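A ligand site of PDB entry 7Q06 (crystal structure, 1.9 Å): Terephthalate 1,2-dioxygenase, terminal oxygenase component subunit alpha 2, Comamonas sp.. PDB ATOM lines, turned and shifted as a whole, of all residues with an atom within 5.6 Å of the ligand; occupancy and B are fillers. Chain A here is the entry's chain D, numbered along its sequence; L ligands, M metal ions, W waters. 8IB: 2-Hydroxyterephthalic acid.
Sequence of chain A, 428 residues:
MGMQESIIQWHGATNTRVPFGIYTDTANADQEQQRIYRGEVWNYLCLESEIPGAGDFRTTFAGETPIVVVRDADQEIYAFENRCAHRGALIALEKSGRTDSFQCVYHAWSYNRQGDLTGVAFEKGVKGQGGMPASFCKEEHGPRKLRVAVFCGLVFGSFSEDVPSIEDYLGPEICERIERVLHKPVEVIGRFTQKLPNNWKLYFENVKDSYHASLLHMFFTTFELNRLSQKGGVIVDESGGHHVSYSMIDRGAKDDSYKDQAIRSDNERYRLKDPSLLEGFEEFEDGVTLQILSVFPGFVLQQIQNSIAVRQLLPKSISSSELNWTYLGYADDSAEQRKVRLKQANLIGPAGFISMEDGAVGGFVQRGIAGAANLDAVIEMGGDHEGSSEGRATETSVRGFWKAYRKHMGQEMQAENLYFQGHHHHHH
The guanidinium group of Arg 311 is in salt-bridge range of an oxygen (O4) of the ligand (2.7 Å). An oxygen (O2) of the ligand lies within hydrogen-bond range of the side-chain hydroxyl (OG) of Ser 245 (2.5 Å). The guanidinium group of Arg 392 lies within salt-bridge range of an oxygen (O1) of the ligand, at 3.6 Å. The side-chain amide nitrogen (ND2) of Asn 226 is in hydrogen-bond range of an oxygen (O1) of the ligand (2.8 Å).
N of Asn 226 lies within hydrogen-bond range of O of Phe 220 (3.0 Å). The side-chain hydroxyl (OG) of Ser 210 sits at hydrogen-bond distance from the backbone carbonyl oxygen (O) of Arg 392, 2.9 Å away. N of Ser 245 lies within hydrogen-bond range of O of Ile 292, 2.9 Å away. The guanidinium group (NH2) of Arg 311 lies within hydrogen-bond range of the side-chain hydroxyl (OH) of Tyr 203, at 2.9 Å. The side-chain amide oxygen of Asn 226 lies within hydrogen-bond range of the guanidinium group of Arg 392, at 2.8 Å. The guanidinium group (NH1) of Arg 311 is in hydrogen-bond range of the side-chain amide oxygen (OE1) of Gln 302 (2.9 Å).
Residues that only touch the ligand: Val 207, Ser 210, Ala 213, Phe 220, Leu 290, Ile 292 and Ile 304. Hydrophobic or aromatic side chains that line the ligand: Ala 213, Phe 220, Leu 290, Ile 292 and Ile 304. 11 residues have an atom within 4 Å of the ligand: Val 207, Ser 210, Ala 213, Phe 220, Asn 226, Ser 245, Leu 290, Ile 292, Ile 304, Arg 311 and Arg 392. The nearest printed residue that does not touch the ligand is Asp 358 (4.1 Å).
Water W2 lies within hydrogen-bond range of an oxygen (O1) of the ligand (2.7 Å), the guanidinium group of Arg 392 (2.9 Å) and the backbone carbonyl oxygen of Ser 210 (3.0 Å). Water W1 lies within hydrogen-bond range of the side-chain carboxylate of Asp 358, the side-chain hydroxyl of Ser 355 and an oxygen (O5) of the ligand.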
ATOM      1  N   TYR A 203      11.323 -19.337 -12.120  1.00  0.00           N
ATOM      2  CA  TYR A 203      12.288 -19.532 -13.220  1.00  0.00           C
ATOM      3  C   TYR A 203      13.403 -20.474 -12.724  1.00  0.00           C
ATOM      4  O   TYR A 203      13.778 -21.445 -13.421  1.00  0.00           O
ATOM      5  CB  TYR A 203      12.900 -18.244 -13.779  1.00  0.00           C
ATOM      6  CG  TYR A 203      13.875 -18.596 -14.896  1.00  0.00           C
ATOM      7  CD1 TYR A 203      13.429 -18.923 -16.158  1.00  0.00           C
ATOM      8  CD2 TYR A 203      15.228 -18.668 -14.661  1.00  0.00           C
ATOM      9  CE1 TYR A 203      14.320 -19.272 -17.175  1.00  0.00           C
ATOM     10  CE2 TYR A 203      16.119 -19.037 -15.633  1.00  0.00           C
ATOM     11  CZ  TYR A 203      15.680 -19.320 -16.906  1.00  0.00           C
ATOM     12  OH  TYR A 203      16.579 -19.677 -17.864  1.00  0.00           O
ATOM     13  N   ASN A 206      12.235 -23.862 -12.682  1.00  0.00           N
ATOM     14  CA  ASN A 206      12.112 -24.300 -14.099  1.00  0.00           C
ATOM     15  C   ASN A 206      13.484 -24.815 -14.621  1.00  0.00           C
ATOM     16  O   ASN A 206      13.501 -25.852 -15.264  1.00  0.00           O
ATOM     17  CB  ASN A 206      11.561 -23.178 -14.970  1.00  0.00           C
ATOM     18  CG  ASN A 206      11.285 -23.646 -16.377  1.00  0.00           C
ATOM     19  OD1 ASN A 206      10.326 -24.365 -16.594  1.00  0.00           O
ATOM     20  ND2 ASN A 206      12.154 -23.332 -17.298  1.00  0.00           N
ATOM     21  N   VAL A 207      14.571 -24.108 -14.351  1.00  0.00           N
ATOM     22  CA  VAL A 207      15.936 -24.508 -14.808  1.00  0.00           C
ATOM     23  C   VAL A 207      16.272 -25.900 -14.245  1.00  0.00           C
ATOM     24  O   VAL A 207      16.922 -26.711 -14.943  1.00  0.00           O
ATOM     25  CB  VAL A 207      17.005 -23.476 -14.376  1.00  0.00           C
ATOM     26  CG1 VAL A 207      18.369 -23.966 -14.744  1.00  0.00           C
ATOM     27  CG2 VAL A 207      16.792 -22.137 -15.005  1.00  0.00           C
ATOM     28  N   LYS A 208      15.848 -26.167 -13.015  1.00  0.00           N
ATOM     29  CA  LYS A 208      16.129 -27.427 -12.262  1.00  0.00           C
ATOM     30  C   LYS A 208      15.123 -28.513 -12.656  1.00  0.00           C
ATOM     31  O   LYS A 208      15.269 -29.640 -12.124  1.00  0.00           O
ATOM     32  CB  LYS A 208      16.086 -27.127 -10.767  1.00  0.00           C
ATOM     33  CG  LYS A 208      17.188 -26.190 -10.287  1.00  0.00           C
ATOM     34  CD  LYS A 208      17.032 -25.715  -8.888  1.00  0.00           C
ATOM     35  CE  LYS A 208      18.180 -24.848  -8.404  1.00  0.00           C
ATOM     36  NZ  LYS A 208      19.442 -25.621  -8.326  1.00  0.00           N
ATOM     37  N   ASP A 209      14.147 -28.214 -13.499  1.00  0.00           N
ATOM     38  CA  ASP A 209      13.008 -29.128 -13.682  1.00  0.00           C
ATOM     39  C   ASP A 209      13.323 -30.063 -14.841  1.00  0.00           C
ATOM     40  O   ASP A 209      12.921 -29.767 -15.968  1.00  0.00           O
ATOM     41  CB  ASP A 209      11.703 -28.319 -13.780  1.00  0.00           C
ATOM     42  CG  ASP A 209      10.421 -29.123 -13.877  1.00  0.00           C
ATOM     43  OD1 ASP A 209      10.476 -30.359 -14.051  1.00  0.00           O
ATOM     44  OD2 ASP A 209       9.379 -28.483 -13.851  1.00  0.00           O
ATOM     45  N   SER A 210      13.993 -31.200 -14.559  1.00  0.00           N
ATOM     46  CA  SER A 210      14.383 -32.201 -15.592  1.00  0.00           C
ATOM     47  C   SER A 210      13.109 -32.803 -16.157  1.00  0.00           C
ATOM     48  O   SER A 210      13.078 -33.098 -17.363  1.00  0.00           O
ATOM     49  CB  SER A 210      15.315 -33.256 -15.029  1.00  0.00           C
ATOM     50  OG  SER A 210      14.753 -33.897 -13.849  1.00  0.00           O
ATOM     51  N   HIS A 212      10.166 -31.418 -16.867  1.00  0.00           N
ATOM     52  CA  HIS A 212       9.487 -30.618 -17.922  1.00  0.00           C
ATOM     53  C   HIS A 212      10.245 -30.635 -19.255  1.00  0.00           C
ATOM     54  O   HIS A 212       9.578 -30.415 -20.257  1.00  0.00           O
ATOM     55  CB  HIS A 212       9.199 -29.161 -17.451  1.00  0.00           C
ATOM     56  CG  HIS A 212      10.197 -28.177 -17.885  1.00  0.00           C
ATOM     57  ND1 HIS A 212      11.403 -28.019 -17.209  1.00  0.00           N
ATOM     58  CD2 HIS A 212      10.172 -27.271 -18.906  1.00  0.00           C
ATOM     59  CE1 HIS A 212      12.120 -27.072 -17.810  1.00  0.00           C
ATOM     60  NE2 HIS A 212      11.353 -26.586 -18.867  1.00  0.00           N
ATOM     61  N   ALA A 213      11.574 -30.798 -19.297  1.00  0.00           N
ATOM     62  CA  ALA A 213      12.384 -30.456 -20.505  1.00  0.00           C
ATOM     63  C   ALA A 213      11.818 -31.060 -21.810  1.00  0.00           C
ATOM     64  O   ALA A 213      11.703 -30.326 -22.822  1.00  0.00           O
ATOM     65  CB  ALA A 213      13.814 -30.857 -20.278  1.00  0.00           C
ATOM     66  N   PHE A 220      12.932 -30.467 -28.092  1.00  0.00           N
ATOM     67  CA  PHE A 220      13.764 -31.465 -27.337  1.00  0.00           C
ATOM     68  C   PHE A 220      13.333 -32.929 -27.606  1.00  0.00           C
ATOM     69  O   PHE A 220      14.204 -33.818 -27.513  1.00  0.00           O
ATOM     70  CB  PHE A 220      13.751 -31.241 -25.823  1.00  0.00           C
ATOM     71  CG  PHE A 220      14.789 -30.268 -25.296  1.00  0.00           C
ATOM     72  CD1 PHE A 220      16.010 -30.074 -25.929  1.00  0.00           C
ATOM     73  CD2 PHE A 220      14.534 -29.553 -24.141  1.00  0.00           C
ATOM     74  CE1 PHE A 220      16.949 -29.180 -25.436  1.00  0.00           C
ATOM     75  CE2 PHE A 220      15.478 -28.686 -23.616  1.00  0.00           C
ATOM     76  CZ  PHE A 220      16.682 -28.493 -24.281  1.00  0.00           C
ATOM     77  N   ASN A 226      16.841 -34.425 -26.224  1.00  0.00           N
ATOM     78  CA  ASN A 226      16.707 -34.358 -24.739  1.00  0.00           C
ATOM     79  C   ASN A 226      15.471 -35.110 -24.213  1.00  0.00           C
ATOM     80  O   ASN A 226      14.737 -34.567 -23.316  1.00  0.00           O
ATOM     81  CB  ASN A 226      16.664 -32.902 -24.275  1.00  0.00           C
ATOM     82  CG  ASN A 226      17.065 -32.766 -22.829  1.00  0.00           C
ATOM     83  OD1 ASN A 226      17.795 -33.609 -22.317  1.00  0.00           O
ATOM     84  ND2 ASN A 226      16.595 -31.701 -22.188  1.00  0.00           N
ATOM     85  N   HIS A 243      22.466 -27.859  -9.139  1.00  0.00           N
ATOM     86  CA  HIS A 243      22.143 -29.094  -9.883  1.00  0.00           C
ATOM     87  C   HIS A 243      22.926 -29.110 -11.188  1.00  0.00           C
ATOM     88  O   HIS A 243      23.432 -28.045 -11.658  1.00  0.00           O
ATOM     89  CB  HIS A 243      20.627 -29.314 -10.069  1.00  0.00           C
ATOM     90  CG  HIS A 243      20.101 -28.990 -11.432  1.00  0.00           C
ATOM     91  ND1 HIS A 243      20.230 -27.729 -11.987  1.00  0.00           N
ATOM     92  CD2 HIS A 243      19.438 -29.743 -12.334  1.00  0.00           C
ATOM     93  CE1 HIS A 243      19.669 -27.743 -13.206  1.00  0.00           C
ATOM     94  NE2 HIS A 243      19.173 -28.969 -13.439  1.00  0.00           N
ATOM     95  N   SER A 245      21.688 -31.140 -14.903  1.00  0.00           N
ATOM     96  CA  SER A 245      20.887 -32.086 -15.711  1.00  0.00           C
ATOM     97  C   SER A 245      21.674 -32.322 -16.976  1.00  0.00           C
ATOM     98  O   SER A 245      22.180 -31.327 -17.572  1.00  0.00           O
ATOM     99  CB  SER A 245      19.485 -31.552 -15.936  1.00  0.00           C
ATOM    100  OG  SER A 245      18.771 -32.486 -16.730  1.00  0.00           O
ATOM    101  N   LEU A 290      23.946 -32.307 -23.906  1.00  0.00           N
ATOM    102  CA  LEU A 290      23.243 -31.261 -23.106  1.00  0.00           C
ATOM    103  C   LEU A 290      23.741 -31.292 -21.660  1.00  0.00           C
ATOM    104  O   LEU A 290      23.710 -32.352 -21.016  1.00  0.00           O
ATOM    105  CB  LEU A 290      21.733 -31.501 -23.194  1.00  0.00           C
ATOM    106  CG  LEU A 290      20.883 -30.479 -22.435  1.00  0.00           C
ATOM    107  CD1 LEU A 290      19.673 -30.052 -23.255  1.00  0.00           C
ATOM    108  CD2 LEU A 290      20.451 -31.011 -21.078  1.00  0.00           C
ATOM    109  N   ILE A 292      22.974 -28.632 -18.356  1.00  0.00           N
ATOM    110  CA  ILE A 292      22.445 -27.429 -17.683  1.00  0.00           C
ATOM    111  C   ILE A 292      22.911 -27.515 -16.231  1.00  0.00           C
ATOM    112  O   ILE A 292      22.679 -28.527 -15.587  1.00  0.00           O
ATOM    113  CB  ILE A 292      20.901 -27.356 -17.787  1.00  0.00           C
ATOM    114  CG1 ILE A 292      20.409 -27.543 -19.210  1.00  0.00           C
ATOM    115  CG2 ILE A 292      20.428 -26.024 -17.210  1.00  0.00           C
ATOM    116  CD1 ILE A 292      20.848 -26.405 -20.157  1.00  0.00           C
ATOM    117  N   GLN A 302      25.009 -23.089 -19.380  1.00  0.00           N
ATOM    118  CA  GLN A 302      24.349 -24.009 -20.329  1.00  0.00           C
ATOM    119  C   GLN A 302      25.324 -24.442 -21.420  1.00  0.00           C
ATOM    120  O   GLN A 302      26.059 -23.574 -21.980  1.00  0.00           O
ATOM    121  CB  GLN A 302      23.077 -23.426 -20.976  1.00  0.00           C
ATOM    122  CG  GLN A 302      23.368 -22.426 -22.024  1.00  0.00           C
ATOM    123  CD  GLN A 302      22.382 -22.259 -23.160  1.00  0.00           C
ATOM    124  OE1 GLN A 302      21.295 -21.729 -22.977  1.00  0.00           O
ATOM    125  NE2 GLN A 302      22.905 -22.456 -24.370  1.00  0.00           N
ATOM    126  N   ILE A 304      24.150 -26.582 -24.769  1.00  0.00           N
ATOM    127  CA  ILE A 304      23.150 -27.322 -25.581  1.00  0.00           C
ATOM    128  C   ILE A 304      23.803 -27.496 -26.952  1.00  0.00           C
ATOM    129  O   ILE A 304      23.966 -26.500 -27.643  1.00  0.00           O
ATOM    130  CB  ILE A 304      21.798 -26.562 -25.656  1.00  0.00           C
ATOM    131  CG1 ILE A 304      21.258 -26.253 -24.248  1.00  0.00           C
ATOM    132  CG2 ILE A 304      20.828 -27.339 -26.539  1.00  0.00           C
ATOM    133  CD1 ILE A 304      20.030 -25.326 -24.204  1.00  0.00           C
ATOM    134  N   ARG A 311      23.643 -17.485 -17.674  1.00  0.00           N
ATOM    135  CA  ARG A 311      22.444 -16.699 -17.331  1.00  0.00           C
ATOM    136  C   ARG A 311      22.577 -16.235 -15.898  1.00  0.00           C
ATOM    137  O   ARG A 311      23.036 -17.049 -15.022  1.00  0.00           O
ATOM    138  CB  ARG A 311      21.157 -17.503 -17.481  1.00  0.00           C
ATOM    139  CG  ARG A 311      21.111 -18.396 -18.704  1.00  0.00           C
ATOM    140  CD  ARG A 311      19.870 -19.273 -18.762  1.00  0.00           C
ATOM    141  NE  ARG A 311      20.021 -20.346 -19.731  1.00  0.00           N
ATOM    142  CZ  ARG A 311      19.324 -21.494 -19.749  1.00  0.00           C
ATOM    143  NH1 ARG A 311      19.518 -22.376 -20.731  1.00  0.00           N
ATOM    144  NH2 ARG A 311      18.344 -21.725 -18.893  1.00  0.00           N
ATOM    145  N   ILE A 354      13.591 -23.479 -27.855  1.00  0.00           N
ATOM    146  CA  ILE A 354      13.392 -24.014 -26.483  1.00  0.00           C
ATOM    147  C   ILE A 354      12.972 -22.882 -25.557  1.00  0.00           C
ATOM    148  O   ILE A 354      11.910 -22.918 -24.931  1.00  0.00           O
ATOM    149  CB  ILE A 354      14.717 -24.594 -25.951  1.00  0.00           C
ATOM    150  CG1 ILE A 354      15.323 -25.651 -26.872  1.00  0.00           C
ATOM    151  CG2 ILE A 354      14.513 -25.085 -24.528  1.00  0.00           C
ATOM    152  CD1 ILE A 354      14.330 -26.631 -27.376  1.00  0.00           C
ATOM    153  N   SER A 355      13.859 -21.929 -25.382  1.00  0.00           N
ATOM    154  CA  SER A 355      13.855 -21.025 -24.212  1.00  0.00           C
ATOM    155  C   SER A 355      12.635 -20.078 -24.217  1.00  0.00           C
ATOM    156  O   SER A 355      12.331 -19.534 -23.148  1.00  0.00           O
ATOM    157  CB  SER A 355      15.138 -20.240 -24.240  1.00  0.00           C
ATOM    158  OG  SER A 355      16.257 -21.112 -24.129  1.00  0.00           O
ATOM    159  N   ASP A 358      10.185 -21.262 -21.806  1.00  0.00           N
ATOM    160  CA  ASP A 358      10.673 -21.142 -20.409  1.00  0.00           C
ATOM    161  C   ASP A 358      10.391 -19.724 -19.923  1.00  0.00           C
ATOM    162  O   ASP A 358      10.069 -19.579 -18.738  1.00  0.00           O
ATOM    163  CB  ASP A 358      12.148 -21.520 -20.226  1.00  0.00           C
ATOM    164  CG  ASP A 358      12.468 -22.980 -20.528  1.00  0.00           C
ATOM    165  OD1 ASP A 358      11.710 -23.865 -20.097  1.00  0.00           O
ATOM    166  OD2 ASP A 358      13.483 -23.214 -21.186  1.00  0.00           O
ATOM    167  N   ARG A 392      15.578 -38.845 -15.522  1.00  0.00           N
ATOM    168  CA  ARG A 392      15.214 -37.417 -15.452  1.00  0.00           C
ATOM    169  C   ARG A 392      13.705 -37.268 -15.214  1.00  0.00           C
ATOM    170  O   ARG A 392      13.277 -36.066 -15.061  1.00  0.00           O
ATOM    171  CB  ARG A 392      15.780 -36.766 -16.712  1.00  0.00           C
ATOM    172  CG  ARG A 392      17.237 -36.327 -16.521  1.00  0.00           C
ATOM    173  CD  ARG A 392      18.270 -36.653 -17.592  1.00  0.00           C
ATOM    174  NE  ARG A 392      17.748 -36.886 -18.918  1.00  0.00           N
ATOM    175  CZ  ARG A 392      17.731 -36.005 -19.924  1.00  0.00           C
ATOM    176  NH1 ARG A 392      18.230 -34.769 -19.771  1.00  0.00           N
ATOM    177  NH2 ARG A 392      17.203 -36.388 -21.080  1.00  0.00           N
HETATM  178  C1  8IB L   1      16.629 -28.120 -17.944  1.00  0.00           C
HETATM  179  C2  8IB L   1      16.670 -26.780 -18.261  1.00  0.00           C
HETATM  180  C3  8IB L   1      17.000 -26.347 -19.550  1.00  0.00           C
HETATM  181  C4  8IB L   1      17.314 -27.314 -20.513  1.00  0.00           C
HETATM  182  C5  8IB L   1      17.279 -28.669 -20.185  1.00  0.00           C
HETATM  183  C6  8IB L   1      16.922 -29.092 -18.905  1.00  0.00           C
HETATM  184  C7  8IB L   1      16.916 -30.585 -18.536  1.00  0.00           C
HETATM  185  O1  8IB L   1      16.915 -31.441 -19.461  1.00  0.00           O
HETATM  186  O2  8IB L   1      16.953 -30.870 -17.331  1.00  0.00           O
HETATM  187  O3  8IB L   1      17.654 -26.949 -21.779  1.00  0.00           O
HETATM  188  C8  8IB L   1      17.096 -24.873 -19.897  1.00  0.00           C
HETATM  189  O4  8IB L   1      16.847 -24.026 -18.996  1.00  0.00           O
HETATM  190  O5  8IB L   1      17.521 -24.564 -21.063  1.00  0.00           O
HETATM  191 FE    FE M   1      13.507 -25.944 -20.285  1.00  0.00          FE
HETATM  192  O   HOH W   1      15.770 -22.362 -21.652  1.00  0.00           O
HETATM  193  O   HOH W   2      15.595 -33.761 -18.925  1.00  0.00           O
